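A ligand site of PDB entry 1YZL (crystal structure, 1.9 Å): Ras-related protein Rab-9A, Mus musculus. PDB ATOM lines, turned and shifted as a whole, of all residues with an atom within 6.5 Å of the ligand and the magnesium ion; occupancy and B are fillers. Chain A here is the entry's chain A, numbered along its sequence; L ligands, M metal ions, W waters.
The backbone NH (N) of Gly 21 sits close to a nitrogen (N1) of the ligand (3.1 Å). Asp 19 touches the ligand (O to O4, 3.9 Å). Gly 20 touches the ligand. Phe 36 touches the ligand (CZ to O12, 3.3 Å). Leu 40 touches the ligand (CB to O8, 3.5 Å). O of Thr 67 touches O3 of the ligand, 3.9 Å away. C of Ala 68 touches O3 of the ligand (3.8 Å). Ile 132 touches the ligand (CD1 to N5, 3.8 Å). Hydrophobic or aromatic side chains within 4 Å of the ligand: Val 22, Phe 36, Leu 40, His 42, Ile 132 and Ala 159. 24 residues have an atom within 4 Å of the ligand: Asp 19, Gly 20, Gly 21, Val 22, Gly 23, Lys 24, Ser 25, Ser 26, Phe 36, Asp 37, Ser 38, Leu 40, His 42, Thr 43, Thr 67, Ala 68, Gly 69, Asn 128, Lys 129, Asp 131, Ile 132, Ser 158, Ala 159 and Lys 160.
Water W1 bridges an oxygen (O8) of the ligand (2.7 Å) and the backbone carbonyl oxygen of Phe 41 (2.7 Å). Water W8 lies within hydrogen-bond range of the backbone carbonyl oxygen of Thr 67 (2.6 Å) and the side-chain carboxylate of Asp 66 (2.6 Å). Water W6 lies within hydrogen-bond range of O1 of the ligand (2.8 Å), O of Thr 43 (2.8 Å), N of Gln 70 (3.3 Å) and N of Gly 69 (3.4 Å). Water W4 lies within hydrogen-bond range of NZ of Lys 129 (2.9 Å) and N6 of the ligand (3.0 Å). Water W2 bridges O of Ser 38 (2.8 Å) and O11 of the ligand (3.2 Å). Water W7 bridges NZ of Lys 129 and O of Gly 21.
Asp 66 touches the magnesium ion (OD2 to MG, 3.99 Å). The nearest printed residue that does not touch the magnesium ion is Thr 67 (4.5 Å).
The magnesium ion is bound by an oxygen (O2) of the ligand, the side-chain hydroxyl (OG) of Ser 25, an oxygen (O5) of the ligand, water W8, the side-chain hydroxyl (OG1) of Thr 43 and water W1.
The side-chain carboxylate of Asp 37 sits at hydrogen-bond distance from the backbone NH of Gln 39, 2.8 Å away. NZ of Lys 129 is in hydrogen-bond range of O of Gly 21, at 2.7 Å. The backbone NH (N) of Lys 160 sits close to the side-chain hydroxyl (OG) of Ser 158 (3.3 Å). The backbone NH of Lys 129 lies within hydrogen-bond range of the backbone carbonyl oxygen of Thr 157 (3.0 Å). The backbone NH (N) of Ala 159 sits close to the side-chain amide nitrogen (ND2) of Asn 128 (3.3 Å). N of Asp 161 lies within hydrogen-bond range of OG of Ser 158, at 3.1 Å. A ring nitrogen (NE2) of His 42 lies close to the side-chain amide nitrogen of Gln 70 (3.3 Å). O of Asp 19 sits at hydrogen-bond distance from NZ of Lys 24, at 2.9 Å.
The side-chain hydroxyl (OG) of Ser 26 lies within hydrogen-bond range of an oxygen (O7) of the ligand (2.7 Å). N of Lys 24 is in hydrogen-bond range of O4 of the ligand (2.9 Å). The side-chain hydroxyl (OG) of Ser 158 is in hydrogen-bond range of an oxygen (O13) of the ligand, at 3.3 Å. ND1 of His 42 sits at hydrogen-bond distance from O1 of the ligand, 2.7 Å away. O13 of the ligand is in hydrogen-bond range of N of Ala 159, 2.9 Å away. O5 of the ligand lies close to N of Ser 25, 3.0 Å away. O of Ser 38 is in hydrogen-bond range of O11 of the ligand (3.0 Å). O of Asp 37 sits at hydrogen-bond distance from O12 of the ligand (2.8 Å). An oxygen (O4) of the ligand sits at hydrogen-bond distance from the backbone NH of Gly 23. O10 of the ligand lies within hydrogen-bond range of NZ of Lys 129 (3.0 Å). An oxygen (O2) of the ligand sits close to the backbone NH (N) of Thr 43, 2.7 Å away. An oxygen (O7) of the ligand is in hydrogen-bond range of the backbone NH of Ser 26, 2.9 Å away. OD2 of Asp 131 sits at hydrogen-bond distance from N5 of the ligand (2.9 Å). An oxygen (O3) of the ligand lies within salt-bridge range of the side-chain amino group (NZ) of Lys 24 (2.6 Å). The side-chain amide oxygen (OD1) of Asn 128 sits close to a nitrogen (N3) of the ligand (3.2 Å). N of Gly 69 lies within hydrogen-bond range of O3 of the ligand, at 2.8 Å. O13 of the ligand sits at hydrogen-bond distance from N of Lys 160 (3.3 Å). N of Val 22 lies within hydrogen-bond range of O4 of the ligand, at 3.4 Å.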
ATOM      1  N   GLY A  18      -2.858  27.229 -10.520  1.00  0.00           N
ATOM      2  CA  GLY A  18      -3.314  27.643  -9.193  1.00  0.00           C
ATOM      3  C   GLY A  18      -2.953  29.077  -8.912  1.00  0.00           C
ATOM      4  O   GLY A  18      -2.113  29.643  -9.601  1.00  0.00           O
ATOM      5  N   ASP A  19      -3.564  29.667  -7.879  1.00  0.00           N
ATOM      6  CA  ASP A  19      -3.351  31.077  -7.556  1.00  0.00           C
ATOM      7  C   ASP A  19      -1.886  31.405  -7.344  1.00  0.00           C
ATOM      8  O   ASP A  19      -1.071  30.537  -7.011  1.00  0.00           O
ATOM      9  CB  ASP A  19      -4.136  31.488  -6.288  1.00  0.00           C
ATOM     10  CG  ASP A  19      -5.623  31.711  -6.551  1.00  0.00           C
ATOM     11  OD1 ASP A  19      -6.137  31.396  -7.633  1.00  0.00           O
ATOM     12  OD2 ASP A  19      -6.294  32.223  -5.624  1.00  0.00           O
ATOM     13  N   GLY A  20      -1.542  32.675  -7.504  1.00  0.00           N
ATOM     14  CA  GLY A  20      -0.216  33.157  -7.168  1.00  0.00           C
ATOM     15  C   GLY A  20       0.058  32.887  -5.693  1.00  0.00           C
ATOM     16  O   GLY A  20      -0.809  33.092  -4.836  1.00  0.00           O
ATOM     17  N   GLY A  21       1.250  32.385  -5.404  1.00  0.00           N
ATOM     18  CA  GLY A  21       1.707  32.196  -4.032  1.00  0.00           C
ATOM     19  C   GLY A  21       1.400  30.844  -3.416  1.00  0.00           C
ATOM     20  O   GLY A  21       1.855  30.561  -2.315  1.00  0.00           O
ATOM     21  N   VAL A  22       0.658  29.994  -4.121  1.00  0.00           N
ATOM     22  CA  VAL A  22       0.235  28.711  -3.532  1.00  0.00           C
ATOM     23  C   VAL A  22       1.379  27.714  -3.422  1.00  0.00           C
ATOM     24  O   VAL A  22       1.312  26.804  -2.605  1.00  0.00           O
ATOM     25  CB  VAL A  22      -0.957  28.064  -4.280  1.00  0.00           C
ATOM     26  CG1 VAL A  22      -2.159  29.003  -4.294  1.00  0.00           C
ATOM     27  CG2 VAL A  22      -0.569  27.629  -5.716  1.00  0.00           C
ATOM     28  N   GLY A  23       2.413  27.875  -4.254  1.00  0.00           N
ATOM     29  CA  GLY A  23       3.618  27.041  -4.165  1.00  0.00           C
ATOM     30  C   GLY A  23       3.921  26.158  -5.373  1.00  0.00           C
ATOM     31  O   GLY A  23       4.626  25.178  -5.242  1.00  0.00           O
ATOM     32  N   LYS A  24       3.429  26.533  -6.548  1.00  0.00           N
ATOM     33  CA  LYS A  24       3.620  25.714  -7.754  1.00  0.00           C
ATOM     34  C   LYS A  24       5.090  25.537  -8.124  1.00  0.00           C
ATOM     35  O   LYS A  24       5.567  24.407  -8.333  1.00  0.00           O
ATOM     36  CB  LYS A  24       2.856  26.318  -8.932  1.00  0.00           C
ATOM     37  CG  LYS A  24       1.349  26.359  -8.721  1.00  0.00           C
ATOM     38  CD  LYS A  24       0.593  27.001  -9.884  1.00  0.00           C
ATOM     39  CE  LYS A  24       0.982  28.463 -10.154  1.00  0.00           C
ATOM     40  NZ  LYS A  24       0.740  29.359  -8.964  1.00  0.00           N
ATOM     41  N   SER A  25       5.817  26.645  -8.227  1.00  0.00           N
ATOM     42  CA  SER A  25       7.238  26.593  -8.542  1.00  0.00           C
ATOM     43  C   SER A  25       8.003  25.782  -7.490  1.00  0.00           C
ATOM     44  O   SER A  25       8.865  24.958  -7.825  1.00  0.00           O
ATOM     45  CB  SER A  25       7.816  28.002  -8.662  1.00  0.00           C
ATOM     46  OG  SER A  25       7.109  28.777  -9.613  1.00  0.00           O
ATOM     47  N   SER A  26       7.686  26.011  -6.209  1.00  0.00           N
ATOM     48  CA  SER A  26       8.316  25.263  -5.121  1.00  0.00           C
ATOM     49  C   SER A  26       8.037  23.765  -5.225  1.00  0.00           C
ATOM     50  O   SER A  26       8.922  22.962  -5.006  1.00  0.00           O
ATOM     51  CB  SER A  26       7.842  25.783  -3.760  1.00  0.00           C
ATOM     52  OG  SER A  26       8.127  27.170  -3.621  1.00  0.00           O
ATOM     53  N   LEU A  27       6.811  23.395  -5.573  1.00  0.00           N
ATOM     54  CA  LEU A  27       6.485  21.978  -5.769  1.00  0.00           C
ATOM     55  C   LEU A  27       7.314  21.353  -6.891  1.00  0.00           C
ATOM     56  O   LEU A  27       7.874  20.263  -6.720  1.00  0.00           O
ATOM     57  CB  LEU A  27       4.981  21.792  -6.013  1.00  0.00           C
ATOM     58  CG  LEU A  27       4.141  21.960  -4.749  1.00  0.00           C
ATOM     59  CD1 LEU A  27       2.689  22.263  -5.079  1.00  0.00           C
ATOM     60  CD2 LEU A  27       4.251  20.727  -3.877  1.00  0.00           C
ATOM     61  N   PHE A  36      14.324  23.700  -1.666  1.00  0.00           N
ATOM     62  CA  PHE A  36      13.267  24.643  -1.310  1.00  0.00           C
ATOM     63  C   PHE A  36      13.869  26.027  -1.059  1.00  0.00           C
ATOM     64  O   PHE A  36      14.967  26.142  -0.523  1.00  0.00           O
ATOM     65  CB  PHE A  36      12.507  24.178  -0.060  1.00  0.00           C
ATOM     66  CG  PHE A  36      11.436  25.131   0.383  1.00  0.00           C
ATOM     67  CD1 PHE A  36      10.234  25.216  -0.298  1.00  0.00           C
ATOM     68  CD2 PHE A  36      11.632  25.951   1.498  1.00  0.00           C
ATOM     69  CE1 PHE A  36       9.239  26.092   0.108  1.00  0.00           C
ATOM     70  CE2 PHE A  36      10.641  26.821   1.917  1.00  0.00           C
ATOM     71  CZ  PHE A  36       9.439  26.904   1.218  1.00  0.00           C
ATOM     72  N   ASP A  37      13.120  27.051  -1.452  1.00  0.00           N
ATOM     73  CA  ASP A  37      13.549  28.435  -1.306  1.00  0.00           C
ATOM     74  C   ASP A  37      12.413  29.226  -0.698  1.00  0.00           C
ATOM     75  O   ASP A  37      11.353  29.363  -1.295  1.00  0.00           O
ATOM     76  CB  ASP A  37      13.921  29.008  -2.680  1.00  0.00           C
ATOM     77  CG  ASP A  37      14.721  30.286  -2.596  1.00  0.00           C
ATOM     78  OD1 ASP A  37      14.507  31.087  -1.649  1.00  0.00           O
ATOM     79  OD2 ASP A  37      15.567  30.505  -3.490  1.00  0.00           O
ATOM     80  N   SER A  38      12.644  29.770   0.502  1.00  0.00           N
ATOM     81  CA  SER A  38      11.631  30.566   1.180  1.00  0.00           C
ATOM     82  C   SER A  38      11.398  31.925   0.503  1.00  0.00           C
ATOM     83  O   SER A  38      10.416  32.603   0.817  1.00  0.00           O
ATOM     84  CB  SER A  38      12.005  30.773   2.644  1.00  0.00           C
ATOM     85  OG  SER A  38      13.227  31.486   2.775  1.00  0.00           O
ATOM     86  N   GLN A  39      12.284  32.311  -0.418  1.00  0.00           N
ATOM     87  CA  GLN A  39      12.266  33.636  -1.040  1.00  0.00           C
ATOM     88  C   GLN A  39      11.974  33.659  -2.552  1.00  0.00           C
ATOM     89  O   GLN A  39      12.358  34.602  -3.248  1.00  0.00           O
ATOM     90  CB  GLN A  39      13.612  34.322  -0.797  1.00  0.00           C
ATOM     91  CG  GLN A  39      14.027  34.390   0.659  1.00  0.00           C
ATOM     92  CD  GLN A  39      13.173  35.336   1.461  1.00  0.00           C
ATOM     93  OE1 GLN A  39      12.502  34.935   2.413  1.00  0.00           O
ATOM     94  NE2 GLN A  39      13.178  36.606   1.080  1.00  0.00           N
ATOM     95  N   LEU A  40      11.289  32.627  -3.067  1.00  0.00           N
ATOM     96  CA  LEU A  40      10.955  32.570  -4.499  1.00  0.00           C
ATOM     97  C   LEU A  40      10.132  33.781  -4.956  1.00  0.00           C
ATOM     98  O   LEU A  40       9.293  34.282  -4.208  1.00  0.00           O
ATOM     99  CB  LEU A  40      10.175  31.287  -4.838  1.00  0.00           C
ATOM    100  CG  LEU A  40      10.941  30.014  -5.193  1.00  0.00           C
ATOM    101  CD1 LEU A  40      10.008  29.051  -5.933  1.00  0.00           C
ATOM    102  CD2 LEU A  40      12.180  30.279  -6.042  1.00  0.00           C
ATOM    103  N   PHE A  41      10.367  34.237  -6.196  1.00  0.00           N
ATOM    104  CA  PHE A  41       9.592  35.330  -6.796  1.00  0.00           C
ATOM    105  C   PHE A  41       8.492  34.801  -7.701  1.00  0.00           C
ATOM    106  O   PHE A  41       8.549  33.660  -8.154  1.00  0.00           O
ATOM    107  CB  PHE A  41      10.494  36.239  -7.621  1.00  0.00           C
ATOM    108  CG  PHE A  41      11.609  36.871  -6.832  1.00  0.00           C
ATOM    109  CD1 PHE A  41      11.329  37.583  -5.666  1.00  0.00           C
ATOM    110  CD2 PHE A  41      12.919  36.784  -7.260  1.00  0.00           C
ATOM    111  CE1 PHE A  41      12.356  38.165  -4.932  1.00  0.00           C
ATOM    112  CE2 PHE A  41      13.947  37.366  -6.527  1.00  0.00           C
ATOM    113  CZ  PHE A  41      13.673  38.057  -5.366  1.00  0.00           C
ATOM    114  N   HIS A  42       7.494  35.642  -7.980  1.00  0.00           N
ATOM    115  CA  HIS A  42       6.366  35.269  -8.831  1.00  0.00           C
ATOM    116  C   HIS A  42       6.857  34.842 -10.220  1.00  0.00           C
ATOM    117  O   HIS A  42       7.793  35.429 -10.771  1.00  0.00           O
ATOM    118  CB  HIS A  42       5.349  36.403  -8.960  1.00  0.00           C
ATOM    119  CG  HIS A  42       4.580  36.687  -7.702  1.00  0.00           C
ATOM    120  ND1 HIS A  42       3.592  35.861  -7.212  1.00  0.00           N
ATOM    121  CD2 HIS A  42       4.652  37.726  -6.831  1.00  0.00           C
ATOM    122  CE1 HIS A  42       3.099  36.371  -6.099  1.00  0.00           C
ATOM    123  NE2 HIS A  42       3.725  37.502  -5.839  1.00  0.00           N
ATOM    124  N   THR A  43       6.204  33.813 -10.764  1.00  0.00           N
ATOM    125  CA  THR A  43       6.496  33.335 -12.105  1.00  0.00           C
ATOM    126  C   THR A  43       5.797  34.235 -13.116  1.00  0.00           C
ATOM    127  O   THR A  43       4.677  34.669 -12.897  1.00  0.00           O
ATOM    128  CB  THR A  43       6.061  31.862 -12.275  1.00  0.00           C
ATOM    129  OG1 THR A  43       6.739  31.057 -11.294  1.00  0.00           O
ATOM    130  CG2 THR A  43       6.381  31.320 -13.676  1.00  0.00           C
ATOM    131  N   ILE A  44       6.483  34.514 -14.216  1.00  0.00           N
ATOM    132  CA  ILE A  44       5.949  35.347 -15.286  1.00  0.00           C
ATOM    133  C   ILE A  44       5.636  34.422 -16.470  1.00  0.00           C
ATOM    134  O   ILE A  44       4.511  33.908 -16.578  1.00  0.00           O
ATOM    135  CB  ILE A  44       6.938  36.495 -15.627  1.00  0.00           C
ATOM    136  CG1 ILE A  44       7.168  37.369 -14.399  1.00  0.00           C
ATOM    137  CG2 ILE A  44       6.423  37.345 -16.795  1.00  0.00           C
ATOM    138  CD1 ILE A  44       8.437  38.199 -14.448  1.00  0.00           C
ATOM    139  N   ASP A  66       5.466  24.670 -15.347  1.00  0.00           N
ATOM    140  CA  ASP A  66       5.143  25.585 -14.275  1.00  0.00           C
ATOM    141  C   ASP A  66       4.588  26.854 -14.930  1.00  0.00           C
ATOM    142  O   ASP A  66       5.098  27.285 -15.977  1.00  0.00           O
ATOM    143  CB  ASP A  66       6.412  25.852 -13.475  1.00  0.00           C
ATOM    144  CG  ASP A  66       6.186  26.751 -12.274  1.00  0.00           C
ATOM    145  OD1 ASP A  66       5.045  26.863 -11.794  1.00  0.00           O
ATOM    146  OD2 ASP A  66       7.201  27.323 -11.800  1.00  0.00           O
ATOM    147  N   THR A  67       3.526  27.416 -14.355  1.00  0.00           N
ATOM    148  CA  THR A  67       2.838  28.573 -14.918  1.00  0.00           C
ATOM    149  C   THR A  67       2.667  29.684 -13.879  1.00  0.00           C
ATOM    150  O   THR A  67       2.708  29.426 -12.672  1.00  0.00           O
ATOM    151  CB  THR A  67       1.435  28.205 -15.452  1.00  0.00           C
ATOM    152  OG1 THR A  67       0.576  27.803 -14.373  1.00  0.00           O
ATOM    153  CG2 THR A  67       1.522  27.078 -16.472  1.00  0.00           C
ATOM    154  N   ALA A  68       2.424  30.903 -14.351  1.00  0.00           N
ATOM    155  CA  ALA A  68       2.097  32.034 -13.482  1.00  0.00           C
ATOM    156  C   ALA A  68       0.697  31.861 -12.917  1.00  0.00           C
ATOM    157  O   ALA A  68      -0.240  31.604 -13.664  1.00  0.00           O
ATOM    158  CB  ALA A  68       2.157  33.317 -14.257  1.00  0.00           C
ATOM    159  N   GLY A  69       0.563  31.979 -11.606  1.00  0.00           N
ATOM    160  CA  GLY A  69      -0.746  31.992 -10.971  1.00  0.00           C
ATOM    161  C   GLY A  69      -1.499  33.317 -11.098  1.00  0.00           C
ATOM    162  O   GLY A  69      -2.725  33.343 -11.036  1.00  0.00           O
ATOM    163  N   GLN A  70      -0.762  34.407 -11.281  1.00  0.00           N
ATOM    164  CA  GLN A  70      -1.366  35.751 -11.276  1.00  0.00           C
ATOM    165  C   GLN A  70      -2.181  36.044 -12.534  1.00  0.00           C
ATOM    166  O   GLN A  70      -1.758  35.732 -13.647  1.00  0.00           O
ATOM    167  CB  GLN A  70      -0.291  36.814 -11.073  1.00  0.00           C
ATOM    168  CG  GLN A  70       0.280  36.828  -9.666  1.00  0.00           C
ATOM    169  CD  GLN A  70       1.242  37.973  -9.411  1.00  0.00           C
ATOM    170  OE1 GLN A  70       1.770  38.585 -10.336  1.00  0.00           O
ATOM    171  NE2 GLN A  70       1.471  38.278  -8.133  1.00  0.00           N
ATOM    172  N   THR A  90      -3.606  23.340  -8.033  1.00  0.00           N
ATOM    173  CA  THR A  90      -2.945  23.579  -6.754  1.00  0.00           C
ATOM    174  C   THR A  90      -3.585  24.742  -5.993  1.00  0.00           C
ATOM    175  O   THR A  90      -3.842  25.812  -6.549  1.00  0.00           O
ATOM    176  CB  THR A  90      -1.458  23.891  -6.986  1.00  0.00           C
ATOM    177  OG1 THR A  90      -0.864  22.855  -7.784  1.00  0.00           O
ATOM    178  CG2 THR A  90      -0.708  23.979  -5.675  1.00  0.00           C
ATOM    179  N   ASN A 128      -1.386  22.605  -0.785  1.00  0.00           N
ATOM    180  CA  ASN A 128       0.017  22.776  -0.431  1.00  0.00           C
ATOM    181  C   ASN A 128       0.156  23.620   0.845  1.00  0.00           C
ATOM    182  O   ASN A 128      -0.808  24.223   1.291  1.00  0.00           O
ATOM    183  CB  ASN A 128       0.756  23.437  -1.594  1.00  0.00           C
ATOM    184  CG  ASN A 128       2.274  23.448  -1.415  1.00  0.00           C
ATOM    185  OD1 ASN A 128       2.921  24.468  -1.628  1.00  0.00           O
ATOM    186  ND2 ASN A 128       2.828  22.308  -1.015  1.00  0.00           N
ATOM    187  N   LYS A 129       1.368  23.622   1.405  1.00  0.00           N
ATOM    188  CA  LYS A 129       1.702  24.358   2.624  1.00  0.00           C
ATOM    189  C   LYS A 129       1.066  23.692   3.835  1.00  0.00           C
ATOM    190  O   LYS A 129       0.769  24.370   4.823  1.00  0.00           O
ATOM    191  CB  LYS A 129       1.322  25.847   2.540  1.00  0.00           C
ATOM    192  CG  LYS A 129       1.833  26.524   1.294  1.00  0.00           C
ATOM    193  CD  LYS A 129       2.017  28.023   1.496  1.00  0.00           C
ATOM    194  CE  LYS A 129       2.314  28.696   0.168  1.00  0.00           C
ATOM    195  NZ  LYS A 129       2.465  30.165   0.284  1.00  0.00           N
ATOM    196  N   THR A 130       0.908  22.375   3.761  1.00  0.00           N
ATOM    197  CA  THR A 130       0.283  21.596   4.845  1.00  0.00           C
ATOM    198  C   THR A 130       1.098  21.691   6.150  1.00  0.00           C
ATOM    199  O   THR A 130       0.570  21.438   7.233  1.00  0.00           O
ATOM    200  CB  THR A 130       0.054  20.120   4.422  1.00  0.00           C
ATOM    201  OG1 THR A 130      -0.997  19.533   5.204  1.00  0.00           O
ATOM    202  CG2 THR A 130       1.329  19.291   4.552  1.00  0.00           C
ATOM    203  N   ASP A 131       2.370  22.068   6.030  1.00  0.00           N
ATOM    204  CA  ASP A 131       3.209  22.359   7.202  1.00  0.00           C
ATOM    205  C   ASP A 131       2.710  23.552   8.037  1.00  0.00           C
ATOM    206  O   ASP A 131       3.070  23.667   9.212  1.00  0.00           O
ATOM    207  CB  ASP A 131       4.652  22.624   6.764  1.00  0.00           C
ATOM    208  CG  ASP A 131       4.764  23.757   5.761  1.00  0.00           C
ATOM    209  OD1 ASP A 131       4.412  23.514   4.588  1.00  0.00           O
ATOM    210  OD2 ASP A 131       5.205  24.857   6.132  1.00  0.00           O
ATOM    211  N   ILE A 132       1.914  24.429   7.450  1.00  0.00           N
ATOM    212  CA  ILE A 132       1.325  25.547   8.186  1.00  0.00           C
ATOM    213  C   ILE A 132       0.100  25.038   8.968  1.00  0.00           C
ATOM    214  O   ILE A 132      -0.866  24.559   8.385  1.00  0.00           O
ATOM    215  CB  ILE A 132       0.961  26.701   7.237  1.00  0.00           C
ATOM    216  CG1 ILE A 132       2.234  27.222   6.541  1.00  0.00           C
ATOM    217  CG2 ILE A 132       0.250  27.841   8.000  1.00  0.00           C
ATOM    218  CD1 ILE A 132       1.993  28.279   5.494  1.00  0.00           C
ATOM    219  N   THR A 157       0.127  18.547   0.617  1.00  0.00           N
ATOM    220  CA  THR A 157       1.551  18.574   0.298  1.00  0.00           C
ATOM    221  C   THR A 157       2.274  19.694   1.016  1.00  0.00           C
ATOM    222  O   THR A 157       1.669  20.678   1.441  1.00  0.00           O
ATOM    223  CB  THR A 157       1.789  18.763  -1.233  1.00  0.00           C
ATOM    224  OG1 THR A 157       1.350  20.069  -1.625  1.00  0.00           O
ATOM    225  CG2 THR A 157       1.052  17.714  -2.037  1.00  0.00           C
ATOM    226  N   SER A 158       3.580  19.526   1.153  1.00  0.00           N
ATOM    227  CA  SER A 158       4.452  20.613   1.584  1.00  0.00           C
ATOM    228  C   SER A 158       5.727  20.562   0.760  1.00  0.00           C
ATOM    229  O   SER A 158       6.481  19.585   0.838  1.00  0.00           O
ATOM    230  CB  SER A 158       4.773  20.514   3.072  1.00  0.00           C
ATOM    231  OG  SER A 158       5.668  21.544   3.466  1.00  0.00           O
ATOM    232  N   ALA A 159       5.948  21.584  -0.057  1.00  0.00           N
ATOM    233  CA  ALA A 159       7.224  21.726  -0.771  1.00  0.00           C
ATOM    234  C   ALA A 159       8.327  22.013   0.241  1.00  0.00           C
ATOM    235  O   ALA A 159       9.487  21.690   0.010  1.00  0.00           O
ATOM    236  CB  ALA A 159       7.140  22.847  -1.792  1.00  0.00           C
ATOM    237  N   LYS A 160       7.968  22.627   1.365  1.00  0.00           N
ATOM    238  CA  LYS A 160       8.945  22.998   2.395  1.00  0.00           C
ATOM    239  C   LYS A 160       9.560  21.767   3.077  1.00  0.00           C
ATOM    240  O   LYS A 160      10.790  21.648   3.118  1.00  0.00           O
ATOM    241  CB  LYS A 160       8.300  23.913   3.431  1.00  0.00           C
ATOM    242  CG  LYS A 160       9.277  24.414   4.481  1.00  0.00           C
ATOM    243  CD  LYS A 160       8.603  25.364   5.446  1.00  0.00           C
ATOM    244  CE  LYS A 160       9.563  25.808   6.535  1.00  0.00           C
ATOM    245  NZ  LYS A 160       8.934  26.823   7.421  1.00  0.00           N
ATOM    246  N   ASP A 161       8.736  20.857   3.584  1.00  0.00           N
ATOM    247  CA  ASP A 161       9.246  19.647   4.236  1.00  0.00           C
ATOM    248  C   ASP A 161       9.091  18.357   3.420  1.00  0.00           C
ATOM    249  O   ASP A 161       9.322  17.261   3.931  1.00  0.00           O
ATOM    250  CB  ASP A 161       8.629  19.480   5.631  1.00  0.00           C
ATOM    251  CG  ASP A 161       7.155  19.161   5.603  1.00  0.00           C
ATOM    252  OD1 ASP A 161       6.703  18.456   4.682  1.00  0.00           O
ATOM    253  OD2 ASP A 161       6.438  19.617   6.521  1.00  0.00           O
HETATM  254  P1  LIG L   1       3.405  32.185  -8.824  1.00  0.00           P
HETATM  255  O1  LIG L   1       3.056  33.636  -8.662  1.00  0.00           O
HETATM  256  O2  LIG L   1       4.710  31.938  -9.538  1.00  0.00           O
HETATM  257  O3  LIG L   1       2.184  31.517  -9.403  1.00  0.00           O
HETATM  258  N1  LIG L   1       3.597  31.592  -7.331  1.00  0.00           N
HETATM  259  P2  LIG L   1       3.891  30.068  -6.927  1.00  0.00           P
HETATM  260  O4  LIG L   1       2.623  29.298  -6.824  1.00  0.00           O
HETATM  261  O5  LIG L   1       4.949  29.529  -7.816  1.00  0.00           O
HETATM  262  O6  LIG L   1       4.467  30.042  -5.483  1.00  0.00           O
HETATM  263  P3  LIG L   1       5.944  29.862  -5.061  1.00  0.00           P
HETATM  264  O7  LIG L   1       6.431  28.486  -5.244  1.00  0.00           O
HETATM  265  O8  LIG L   1       6.767  30.947  -5.642  1.00  0.00           O
HETATM  266  O9  LIG L   1       5.927  30.061  -3.483  1.00  0.00           O
HETATM  267  C1  LIG L   1       5.313  31.215  -2.929  1.00  0.00           C
HETATM  268  C2  LIG L   1       5.785  31.418  -1.498  1.00  0.00           C
HETATM  269  O10 LIG L   1       5.289  30.325  -0.679  1.00  0.00           O
HETATM  270  C3  LIG L   1       7.295  31.427  -1.342  1.00  0.00           C
HETATM  271  O11 LIG L   1       7.657  32.327  -0.306  1.00  0.00           O
HETATM  272  C4  LIG L   1       7.589  29.971  -1.006  1.00  0.00           C
HETATM  273  O12 LIG L   1       8.802  29.804  -0.286  1.00  0.00           O
HETATM  274  C5  LIG L   1       6.375  29.602  -0.151  1.00  0.00           C
HETATM  275  N2  LIG L   1       6.046  28.175  -0.150  1.00  0.00           N
HETATM  276  C6  LIG L   1       5.924  27.331  -1.240  1.00  0.00           C
HETATM  277  N3  LIG L   1       5.623  26.119  -0.910  1.00  0.00           N
HETATM  278  C7  LIG L   1       5.533  26.148   0.482  1.00  0.00           C
HETATM  279  C8  LIG L   1       5.222  25.122   1.426  1.00  0.00           C
HETATM  280  O13 LIG L   1       4.966  23.928   1.235  1.00  0.00           O
HETATM  281  N4  LIG L   1       5.236  25.594   2.740  1.00  0.00           N
HETATM  282  C9  LIG L   1       5.500  26.892   3.104  1.00  0.00           C
HETATM  283  N5  LIG L   1       5.469  27.167   4.424  1.00  0.00           N
HETATM  284  N6  LIG L   1       5.790  27.856   2.239  1.00  0.00           N
HETATM  285  C10 LIG L   1       5.789  27.415   0.952  1.00  0.00           C
HETATM  286 MG    MG M   1       5.788  30.297  -9.547  1.00  0.00          MG
HETATM  287  O   HOH W   1       7.191  31.302  -8.275  1.00  0.00           O
HETATM  288  O   HOH W   2       8.570  32.121   2.798  1.00  0.00           O
HETATM  289  O   HOH W   3       5.639  33.334  -5.828  1.00  0.00           O
HETATM  290  O   HOH W   4       4.277  30.439   2.566  1.00  0.00           O
HETATM  291  O   HOH W   5       8.313  29.595   3.258  1.00  0.00           O
HETATM  292  O   HOH W   6       2.498  34.789 -11.133  1.00  0.00           O
HETATM  293  O   HOH W   7       2.956  33.012  -0.442  1.00  0.00           O
HETATM  294  O   HOH W   8       4.502  29.243 -10.832  1.00  0.00           O
HETATM  295  O   HOH W   9       5.842  29.847   5.349  1.00  0.00           O
HETATM  296  O   HOH W  10       5.751  32.782   2.180  1.00  0.00           O
